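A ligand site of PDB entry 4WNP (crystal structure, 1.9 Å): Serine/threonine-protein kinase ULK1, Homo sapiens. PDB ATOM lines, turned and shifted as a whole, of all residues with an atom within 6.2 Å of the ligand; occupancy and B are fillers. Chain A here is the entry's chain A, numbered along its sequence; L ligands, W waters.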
ATOM      1  N   ILE A  26     -25.112  -1.172 -29.436  1.00  0.00           N
ATOM      2  CA  ILE A  26     -24.953   0.201 -29.932  1.00  0.00           C
ATOM      3  C   ILE A  26     -23.612   0.782 -29.558  1.00  0.00           C
ATOM      4  O   ILE A  26     -22.929   1.397 -30.371  1.00  0.00           O
ATOM      5  CB  ILE A  26     -26.009   1.172 -29.368  1.00  0.00           C
ATOM      6  CG1 ILE A  26     -27.421   0.816 -29.817  1.00  0.00           C
ATOM      7  CG2 ILE A  26     -25.691   2.598 -29.796  1.00  0.00           C
ATOM      8  CD1 ILE A  26     -28.459   1.750 -29.208  1.00  0.00           C
ATOM      9  N   GLY A  27     -23.222   0.601 -28.306  1.00  0.00           N
ATOM     10  CA  GLY A  27     -22.070   1.291 -27.764  1.00  0.00           C
ATOM     11  C   GLY A  27     -21.366   0.539 -26.665  1.00  0.00           C
ATOM     12  O   GLY A  27     -21.962  -0.258 -25.930  1.00  0.00           O
ATOM     13  N   HIS A  28     -20.069   0.812 -26.556  1.00  0.00           N
ATOM     14  CA  HIS A  28     -19.183   0.135 -25.626  1.00  0.00           C
ATOM     15  C   HIS A  28     -18.239   1.165 -25.008  1.00  0.00           C
ATOM     16  O   HIS A  28     -17.601   1.934 -25.736  1.00  0.00           O
ATOM     17  CB  HIS A  28     -18.395  -0.960 -26.361  1.00  0.00           C
ATOM     18  CG  HIS A  28     -17.618  -1.854 -25.461  1.00  0.00           C
ATOM     19  ND1 HIS A  28     -18.193  -2.901 -24.779  1.00  0.00           N
ATOM     20  CD2 HIS A  28     -16.291  -1.898 -25.168  1.00  0.00           C
ATOM     21  CE1 HIS A  28     -17.270  -3.530 -24.073  1.00  0.00           C
ATOM     22  NE2 HIS A  28     -16.108  -2.948 -24.299  1.00  0.00           N
ATOM     23  N   VAL A  34     -24.062  -0.598 -24.167  1.00  0.00           N
ATOM     24  CA  VAL A  34     -25.374  -0.070 -24.575  1.00  0.00           C
ATOM     25  C   VAL A  34     -25.981  -0.893 -25.708  1.00  0.00           C
ATOM     26  O   VAL A  34     -25.322  -1.141 -26.714  1.00  0.00           O
ATOM     27  CB  VAL A  34     -25.260   1.413 -24.997  1.00  0.00           C
ATOM     28  CG1 VAL A  34     -26.644   2.011 -25.260  1.00  0.00           C
ATOM     29  CG2 VAL A  34     -24.556   2.219 -23.883  1.00  0.00           C
ATOM     30  N   VAL A  47     -35.520   2.232 -27.787  1.00  0.00           N
ATOM     31  CA  VAL A  47     -34.830   2.692 -26.594  1.00  0.00           C
ATOM     32  C   VAL A  47     -33.349   2.307 -26.697  1.00  0.00           C
ATOM     33  O   VAL A  47     -32.980   1.484 -27.524  1.00  0.00           O
ATOM     34  CB  VAL A  47     -35.431   2.088 -25.244  1.00  0.00           C
ATOM     35  CG1 VAL A  47     -36.864   2.601 -24.945  1.00  0.00           C
ATOM     36  CG2 VAL A  47     -35.393   0.571 -25.214  1.00  0.00           C
ATOM     37  N   ALA A  48     -32.518   2.944 -25.874  1.00  0.00           N
ATOM     38  CA  ALA A  48     -31.133   2.482 -25.711  1.00  0.00           C
ATOM     39  C   ALA A  48     -30.977   2.037 -24.249  1.00  0.00           C
ATOM     40  O   ALA A  48     -31.258   2.817 -23.367  1.00  0.00           O
ATOM     41  CB  ALA A  48     -30.148   3.585 -26.044  1.00  0.00           C
ATOM     42  N   VAL A  49     -30.566   0.782 -24.031  1.00  0.00           N
ATOM     43  CA  VAL A  49     -30.476   0.230 -22.674  1.00  0.00           C
ATOM     44  C   VAL A  49     -29.015   0.201 -22.271  1.00  0.00           C
ATOM     45  O   VAL A  49     -28.237  -0.493 -22.893  1.00  0.00           O
ATOM     46  CB  VAL A  49     -31.044  -1.229 -22.587  1.00  0.00           C
ATOM     47  CG1 VAL A  49     -31.059  -1.688 -21.116  1.00  0.00           C
ATOM     48  CG2 VAL A  49     -32.443  -1.303 -23.158  1.00  0.00           C
ATOM     49  N   LYS A  50     -28.690   0.979 -21.255  1.00  0.00           N
ATOM     50  CA  LYS A  50     -27.330   1.122 -20.745  1.00  0.00           C
ATOM     51  C   LYS A  50     -27.156   0.133 -19.598  1.00  0.00           C
ATOM     52  O   LYS A  50     -27.971   0.117 -18.695  1.00  0.00           O
ATOM     53  CB  LYS A  50     -27.114   2.577 -20.298  1.00  0.00           C
ATOM     54  CG  LYS A  50     -25.690   3.015 -19.977  1.00  0.00           C
ATOM     55  CD  LYS A  50     -25.653   4.560 -20.061  1.00  0.00           C
ATOM     56  CE  LYS A  50     -24.284   5.105 -19.694  1.00  0.00           C
ATOM     57  NZ  LYS A  50     -24.303   6.599 -19.529  1.00  0.00           N
ATOM     58  N   GLU A  67     -25.665   8.245 -12.309  1.00  0.00           N
ATOM     59  CA  GLU A  67     -26.335   8.826 -13.455  1.00  0.00           C
ATOM     60  C   GLU A  67     -27.854   8.740 -13.303  1.00  0.00           C
ATOM     61  O   GLU A  67     -28.586   9.667 -13.666  1.00  0.00           O
ATOM     62  CB  GLU A  67     -25.902   8.136 -14.764  1.00  0.00           C
ATOM     63  CG  GLU A  67     -26.518   8.777 -15.997  1.00  0.00           C
ATOM     64  CD  GLU A  67     -25.830   8.347 -17.288  1.00  0.00           C
ATOM     65  OE1 GLU A  67     -25.261   7.223 -17.310  1.00  0.00           O
ATOM     66  OE2 GLU A  67     -25.856   9.139 -18.261  1.00  0.00           O
ATOM     67  N   VAL A  80     -30.778  13.720 -23.110  1.00  0.00           N
ATOM     68  CA  VAL A  80     -31.277  12.376 -23.480  1.00  0.00           C
ATOM     69  C   VAL A  80     -32.075  11.843 -22.283  1.00  0.00           C
ATOM     70  O   VAL A  80     -31.595  11.866 -21.156  1.00  0.00           O
ATOM     71  CB  VAL A  80     -30.156  11.374 -23.856  1.00  0.00           C
ATOM     72  CG1 VAL A  80     -30.773  10.052 -24.218  1.00  0.00           C
ATOM     73  CG2 VAL A  80     -29.309  11.906 -25.054  1.00  0.00           C
ATOM     74  N   MET A  96     -33.009   4.398 -21.811  1.00  0.00           N
ATOM     75  CA  MET A  96     -32.842   5.770 -22.313  1.00  0.00           C
ATOM     76  C   MET A  96     -33.605   5.980 -23.614  1.00  0.00           C
ATOM     77  O   MET A  96     -33.811   5.058 -24.387  1.00  0.00           O
ATOM     78  CB  MET A  96     -31.360   6.095 -22.597  1.00  0.00           C
ATOM     79  CG  MET A  96     -30.394   5.841 -21.456  1.00  0.00           C
ATOM     80  SD  MET A  96     -30.756   6.873 -20.052  1.00  0.00           S
ATOM     81  CE  MET A  96     -30.505   8.518 -20.747  1.00  0.00           C
ATOM     82  N   GLU A  97     -33.988   7.226 -23.843  1.00  0.00           N
ATOM     83  CA  GLU A  97     -34.444   7.670 -25.154  1.00  0.00           C
ATOM     84  C   GLU A  97     -33.455   7.253 -26.248  1.00  0.00           C
ATOM     85  O   GLU A  97     -32.242   7.345 -26.057  1.00  0.00           O
ATOM     86  CB  GLU A  97     -34.599   9.191 -25.104  1.00  0.00           C
ATOM     87  CG  GLU A  97     -34.899   9.863 -26.423  1.00  0.00           C
ATOM     88  CD  GLU A  97     -34.943  11.385 -26.261  1.00  0.00           C
ATOM     89  OE1 GLU A  97     -34.534  11.903 -25.165  1.00  0.00           O
ATOM     90  OE2 GLU A  97     -35.384  12.064 -27.220  1.00  0.00           O
ATOM     91  N   TYR A  98     -33.970   6.802 -27.379  1.00  0.00           N
ATOM     92  CA  TYR A  98     -33.112   6.410 -28.501  1.00  0.00           C
ATOM     93  C   TYR A  98     -32.984   7.580 -29.474  1.00  0.00           C
ATOM     94  O   TYR A  98     -34.001   8.167 -29.867  1.00  0.00           O
ATOM     95  CB  TYR A  98     -33.668   5.182 -29.211  1.00  0.00           C
ATOM     96  CG  TYR A  98     -32.839   4.775 -30.435  1.00  0.00           C
ATOM     97  CD1 TYR A  98     -31.602   4.183 -30.284  1.00  0.00           C
ATOM     98  CD2 TYR A  98     -33.308   5.015 -31.734  1.00  0.00           C
ATOM     99  CE1 TYR A  98     -30.833   3.807 -31.393  1.00  0.00           C
ATOM    100  CE2 TYR A  98     -32.543   4.644 -32.849  1.00  0.00           C
ATOM    101  CZ  TYR A  98     -31.305   4.043 -32.662  1.00  0.00           C
ATOM    102  OH  TYR A  98     -30.531   3.665 -33.730  1.00  0.00           O
ATOM    103  N   CYS A  99     -31.758   7.940 -29.818  1.00  0.00           N
ATOM    104  CA  CYS A  99     -31.493   9.039 -30.735  1.00  0.00           C
ATOM    105  C   CYS A  99     -30.928   8.439 -32.014  1.00  0.00           C
ATOM    106  O   CYS A  99     -29.811   7.886 -31.992  1.00  0.00           O
ATOM    107  CB  CYS A  99     -30.508  10.042 -30.108  1.00  0.00           C
ATOM    108  SG  CYS A  99     -31.132  10.772 -28.558  1.00  0.00           S
ATOM    109  N   ASN A 100     -31.681   8.513 -33.116  1.00  0.00           N
ATOM    110  CA  ASN A 100     -31.317   7.726 -34.303  1.00  0.00           C
ATOM    111  C   ASN A 100     -30.190   8.318 -35.124  1.00  0.00           C
ATOM    112  O   ASN A 100     -29.688   7.663 -36.032  1.00  0.00           O
ATOM    113  CB  ASN A 100     -32.522   7.512 -35.212  1.00  0.00           C
ATOM    114  CG  ASN A 100     -33.013   8.809 -35.841  1.00  0.00           C
ATOM    115  OD1 ASN A 100     -33.190   9.801 -35.133  1.00  0.00           O
ATOM    116  ND2 ASN A 100     -33.178   8.823 -37.173  1.00  0.00           N
ATOM    117  N   GLY A 101     -29.804   9.546 -34.821  1.00  0.00           N
ATOM    118  CA  GLY A 101     -28.788  10.246 -35.589  1.00  0.00           C
ATOM    119  C   GLY A 101     -27.359  10.025 -35.135  1.00  0.00           C
ATOM    120  O   GLY A 101     -26.412  10.529 -35.767  1.00  0.00           O
ATOM    121  N   GLY A 102     -27.186   9.269 -34.056  1.00  0.00           N
ATOM    122  CA  GLY A 102     -25.845   8.982 -33.560  1.00  0.00           C
ATOM    123  C   GLY A 102     -25.217  10.205 -32.886  1.00  0.00           C
ATOM    124  O   GLY A 102     -25.910  11.153 -32.537  1.00  0.00           O
ATOM    125  N   ASP A 103     -23.896  10.174 -32.653  1.00  0.00           N
ATOM    126  CA  ASP A 103     -23.326  11.262 -31.871  1.00  0.00           C
ATOM    127  C   ASP A 103     -22.713  12.344 -32.758  1.00  0.00           C
ATOM    128  O   ASP A 103     -22.508  12.158 -33.989  1.00  0.00           O
ATOM    129  CB  ASP A 103     -22.300  10.751 -30.830  1.00  0.00           C
ATOM    130  CG  ASP A 103     -21.015  10.172 -31.447  1.00  0.00           C
ATOM    131  OD1 ASP A 103     -20.536  10.689 -32.448  1.00  0.00           O
ATOM    132  OD2 ASP A 103     -20.455   9.201 -30.889  1.00  0.00           O
ATOM    133  N   ASP A 106     -19.364  11.699 -34.829  1.00  0.00           N
ATOM    134  CA  ASP A 106     -19.502  10.985 -36.106  1.00  0.00           C
ATOM    135  C   ASP A 106     -20.163  11.859 -37.148  1.00  0.00           C
ATOM    136  O   ASP A 106     -19.816  11.837 -38.331  1.00  0.00           O
ATOM    137  CB  ASP A 106     -20.314   9.704 -35.918  1.00  0.00           C
ATOM    138  CG  ASP A 106     -19.544   8.629 -35.185  1.00  0.00           C
ATOM    139  OD1 ASP A 106     -18.307   8.802 -35.024  1.00  0.00           O
ATOM    140  OD2 ASP A 106     -20.151   7.619 -34.799  1.00  0.00           O
ATOM    141  N   GLN A 146     -18.734  13.279 -28.494  1.00  0.00           N
ATOM    142  CA  GLN A 146     -19.253  11.922 -28.342  1.00  0.00           C
ATOM    143  C   GLN A 146     -20.426  11.843 -27.369  1.00  0.00           C
ATOM    144  O   GLN A 146     -21.146  10.851 -27.365  1.00  0.00           O
ATOM    145  CB  GLN A 146     -18.141  10.953 -27.870  1.00  0.00           C
ATOM    146  CG  GLN A 146     -17.006  10.733 -28.934  1.00  0.00           C
ATOM    147  CD  GLN A 146     -15.986  11.903 -28.997  1.00  0.00           C
ATOM    148  OE1 GLN A 146     -16.088  12.910 -28.277  1.00  0.00           O
ATOM    149  NE2 GLN A 146     -14.986  11.760 -29.868  1.00  0.00           N
ATOM    150  N   ASN A 147     -20.568  12.848 -26.518  1.00  0.00           N
ATOM    151  CA  ASN A 147     -21.653  12.881 -25.512  1.00  0.00           C
ATOM    152  C   ASN A 147     -22.779  13.861 -25.903  1.00  0.00           C
ATOM    153  O   ASN A 147     -23.627  14.235 -25.065  1.00  0.00           O
ATOM    154  CB  ASN A 147     -21.072  13.225 -24.130  1.00  0.00           C
ATOM    155  CG  ASN A 147     -20.386  12.024 -23.475  1.00  0.00           C
ATOM    156  OD1 ASN A 147     -20.656  10.890 -23.872  1.00  0.00           O
ATOM    157  ND2 ASN A 147     -19.514  12.265 -22.475  1.00  0.00           N
ATOM    158  N   ILE A 148     -22.764  14.276 -27.170  1.00  0.00           N
ATOM    159  CA  ILE A 148     -23.891  14.998 -27.775  1.00  0.00           C
ATOM    160  C   ILE A 148     -24.555  14.082 -28.805  1.00  0.00           C
ATOM    161  O   ILE A 148     -23.917  13.702 -29.786  1.00  0.00           O
ATOM    162  CB  ILE A 148     -23.430  16.297 -28.494  1.00  0.00           C
ATOM    163  CG1 ILE A 148     -22.674  17.223 -27.545  1.00  0.00           C
ATOM    164  CG2 ILE A 148     -24.626  17.024 -29.110  1.00  0.00           C
ATOM    165  CD1 ILE A 148     -23.513  17.681 -26.357  1.00  0.00           C
ATOM    166  N   LEU A 149     -25.828  13.719 -28.588  1.00  0.00           N
ATOM    167  CA  LEU A 149     -26.499  12.776 -29.457  1.00  0.00           C
ATOM    168  C   LEU A 149     -27.448  13.571 -30.354  1.00  0.00           C
ATOM    169  O   LEU A 149     -27.963  14.606 -29.948  1.00  0.00           O
ATOM    170  CB  LEU A 149     -27.283  11.730 -28.667  1.00  0.00           C
ATOM    171  CG  LEU A 149     -26.504  10.478 -28.231  1.00  0.00           C
ATOM    172  CD1 LEU A 149     -26.253   9.593 -29.452  1.00  0.00           C
ATOM    173  CD2 LEU A 149     -25.194  10.828 -27.566  1.00  0.00           C
ATOM    174  N   ALA A 168     -25.753  13.751 -23.316  1.00  0.00           N
ATOM    175  CA  ALA A 168     -25.729  12.416 -22.751  1.00  0.00           C
ATOM    176  C   ALA A 168     -24.623  12.259 -21.686  1.00  0.00           C
ATOM    177  O   ALA A 168     -23.729  13.108 -21.589  1.00  0.00           O
ATOM    178  CB  ALA A 168     -25.528  11.382 -23.868  1.00  0.00           C
ATOM    179  N   ASP A 169     -24.706  11.165 -20.929  1.00  0.00           N
ATOM    180  CA  ASP A 169     -23.643  10.694 -20.012  1.00  0.00           C
ATOM    181  C   ASP A 169     -23.409  11.571 -18.796  1.00  0.00           C
ATOM    182  O   ASP A 169     -22.468  12.369 -18.764  1.00  0.00           O
ATOM    183  CB  ASP A 169     -22.312  10.526 -20.758  1.00  0.00           C
ATOM    184  CG  ASP A 169     -21.392   9.537 -20.072  1.00  0.00           C
ATOM    185  OD1 ASP A 169     -21.629   9.228 -18.864  1.00  0.00           O
ATOM    186  OD2 ASP A 169     -20.443   9.067 -20.731  1.00  0.00           O
HETATM  187  C1  LIG L   1     -28.332   6.828 -24.918  1.00  0.00           C
HETATM  188  C2  LIG L   1     -26.796   6.688 -23.523  1.00  0.00           C
HETATM  189  C3  LIG L   1     -27.610   6.408 -27.460  1.00  0.00           C
HETATM  190  C4  LIG L   1     -23.400   6.195 -28.125  1.00  0.00           C
HETATM  191  C5  LIG L   1     -22.791   7.378 -27.737  1.00  0.00           C
HETATM  192  C6  LIG L   1     -23.993   5.700 -25.851  1.00  0.00           C
HETATM  193  C7  LIG L   1     -25.420   5.478 -32.479  1.00  0.00           C
HETATM  194  C8  LIG L   1     -25.233   5.179 -33.851  1.00  0.00           C
HETATM  195  C9  LIG L   1     -26.331   5.155 -34.680  1.00  0.00           C
HETATM  196  C10 LIG L   1     -27.622   5.404 -34.174  1.00  0.00           C
HETATM  197  C11 LIG L   1     -27.810   5.686 -32.818  1.00  0.00           C
HETATM  198  C12 LIG L   1     -26.662   5.715 -31.956  1.00  0.00           C
HETATM  199  C13 LIG L   1     -26.775   6.016 -30.571  1.00  0.00           C
HETATM  200  N1  LIG L   1     -28.056   6.268 -30.037  1.00  0.00           N
HETATM  201  C14 LIG L   1     -28.366   6.498 -28.651  1.00  0.00           C
HETATM  202  N2  LIG L   1     -29.635   6.856 -28.331  1.00  0.00           N
HETATM  203  N3  LIG L   1     -29.688   7.031 -26.982  1.00  0.00           N
HETATM  204  C15 LIG L   1     -28.508   6.754 -26.418  1.00  0.00           C
HETATM  205  C16 LIG L   1     -27.653   5.678 -24.212  1.00  0.00           C
HETATM  206  C17 LIG L   1     -27.166   7.685 -24.564  1.00  0.00           C
HETATM  207  N4  LIG L   1     -25.694   6.036 -29.764  1.00  0.00           N
HETATM  208  C18 LIG L   1     -24.486   5.796 -30.314  1.00  0.00           C
HETATM  209  N5  LIG L   1     -23.336   5.853 -29.503  1.00  0.00           N
HETATM  210  C19 LIG L   1     -22.798   7.734 -26.369  1.00  0.00           C
HETATM  211  N6  LIG L   1     -22.302   8.825 -25.718  1.00  0.00           N
HETATM  212  C20 LIG L   1     -22.558   8.689 -24.394  1.00  0.00           C
HETATM  213  N7  LIG L   1     -23.223   7.522 -24.211  1.00  0.00           N
HETATM  214  C21 LIG L   1     -23.379   6.907 -25.443  1.00  0.00           C
HETATM  215  C22 LIG L   1     -23.985   5.346 -27.202  1.00  0.00           C
HETATM  216  N8  LIG L   1     -24.317   5.526 -31.630  1.00  0.00           N
HETATM  217  O   HOH W   1     -21.503   6.145 -32.159  1.00  0.00           O
HETATM  218  O   HOH W   2     -24.377   8.142 -21.668  1.00  0.00           O
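The backbone NH (N) of Cys 99 sits at hydrogen-bond distance from a nitrogen (N2) of the ligand.
A nitrogen (N6) of the ligand sits close to the side-chain amide oxygen of Asn 147 (3.2 Å).
The backbone carbonyl oxygen of Gln 146 sits at hydrogen-bond distance from a nitrogen (N6) of the ligand (2.9 Å).
N1 of the ligand is in hydrogen-bond range of O of Cys 99.
A nitrogen (N3) of the ligand sits at hydrogen-bond distance from the backbone carbonyl oxygen of Glu 97.
N of Ala 168 is in hydrogen-bond range of O of Asn 147, at 2.8 Å.
The backbone NH of Ile 26 sits at hydrogen-bond distance from the backbone carbonyl oxygen of Val 34, 2.7 Å away.
The backbone carbonyl oxygen (O) of Ala 48 is in hydrogen-bond range of the backbone NH (N) of Met 96 (2.8 Å).
The backbone NH (N) of Val 34 lies within hydrogen-bond range of the backbone carbonyl oxygen (O) of Gly 27.
Merely in contact with the ligand: Tyr 98 (3.4 Å), Ile 26 (3.4 Å), Asn 100 (3.6 Å), Ala 48 (3.6 Å), Leu 149 (3.6 Å), Gly 102 (3.7 Å), Met 96 (3.9 Å) and Val 34 (3.9 Å).
Of the 25 residues printed, 12 come within 4 Å of the ligand.
Water W2 lies within hydrogen-bond range of the side-chain amino group (NZ) of Lys 50 (2.6 Å), a nitrogen (N7) of the ligand (2.9 Å) and the backbone NH (N) of Asp 169 (3.1 Å).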
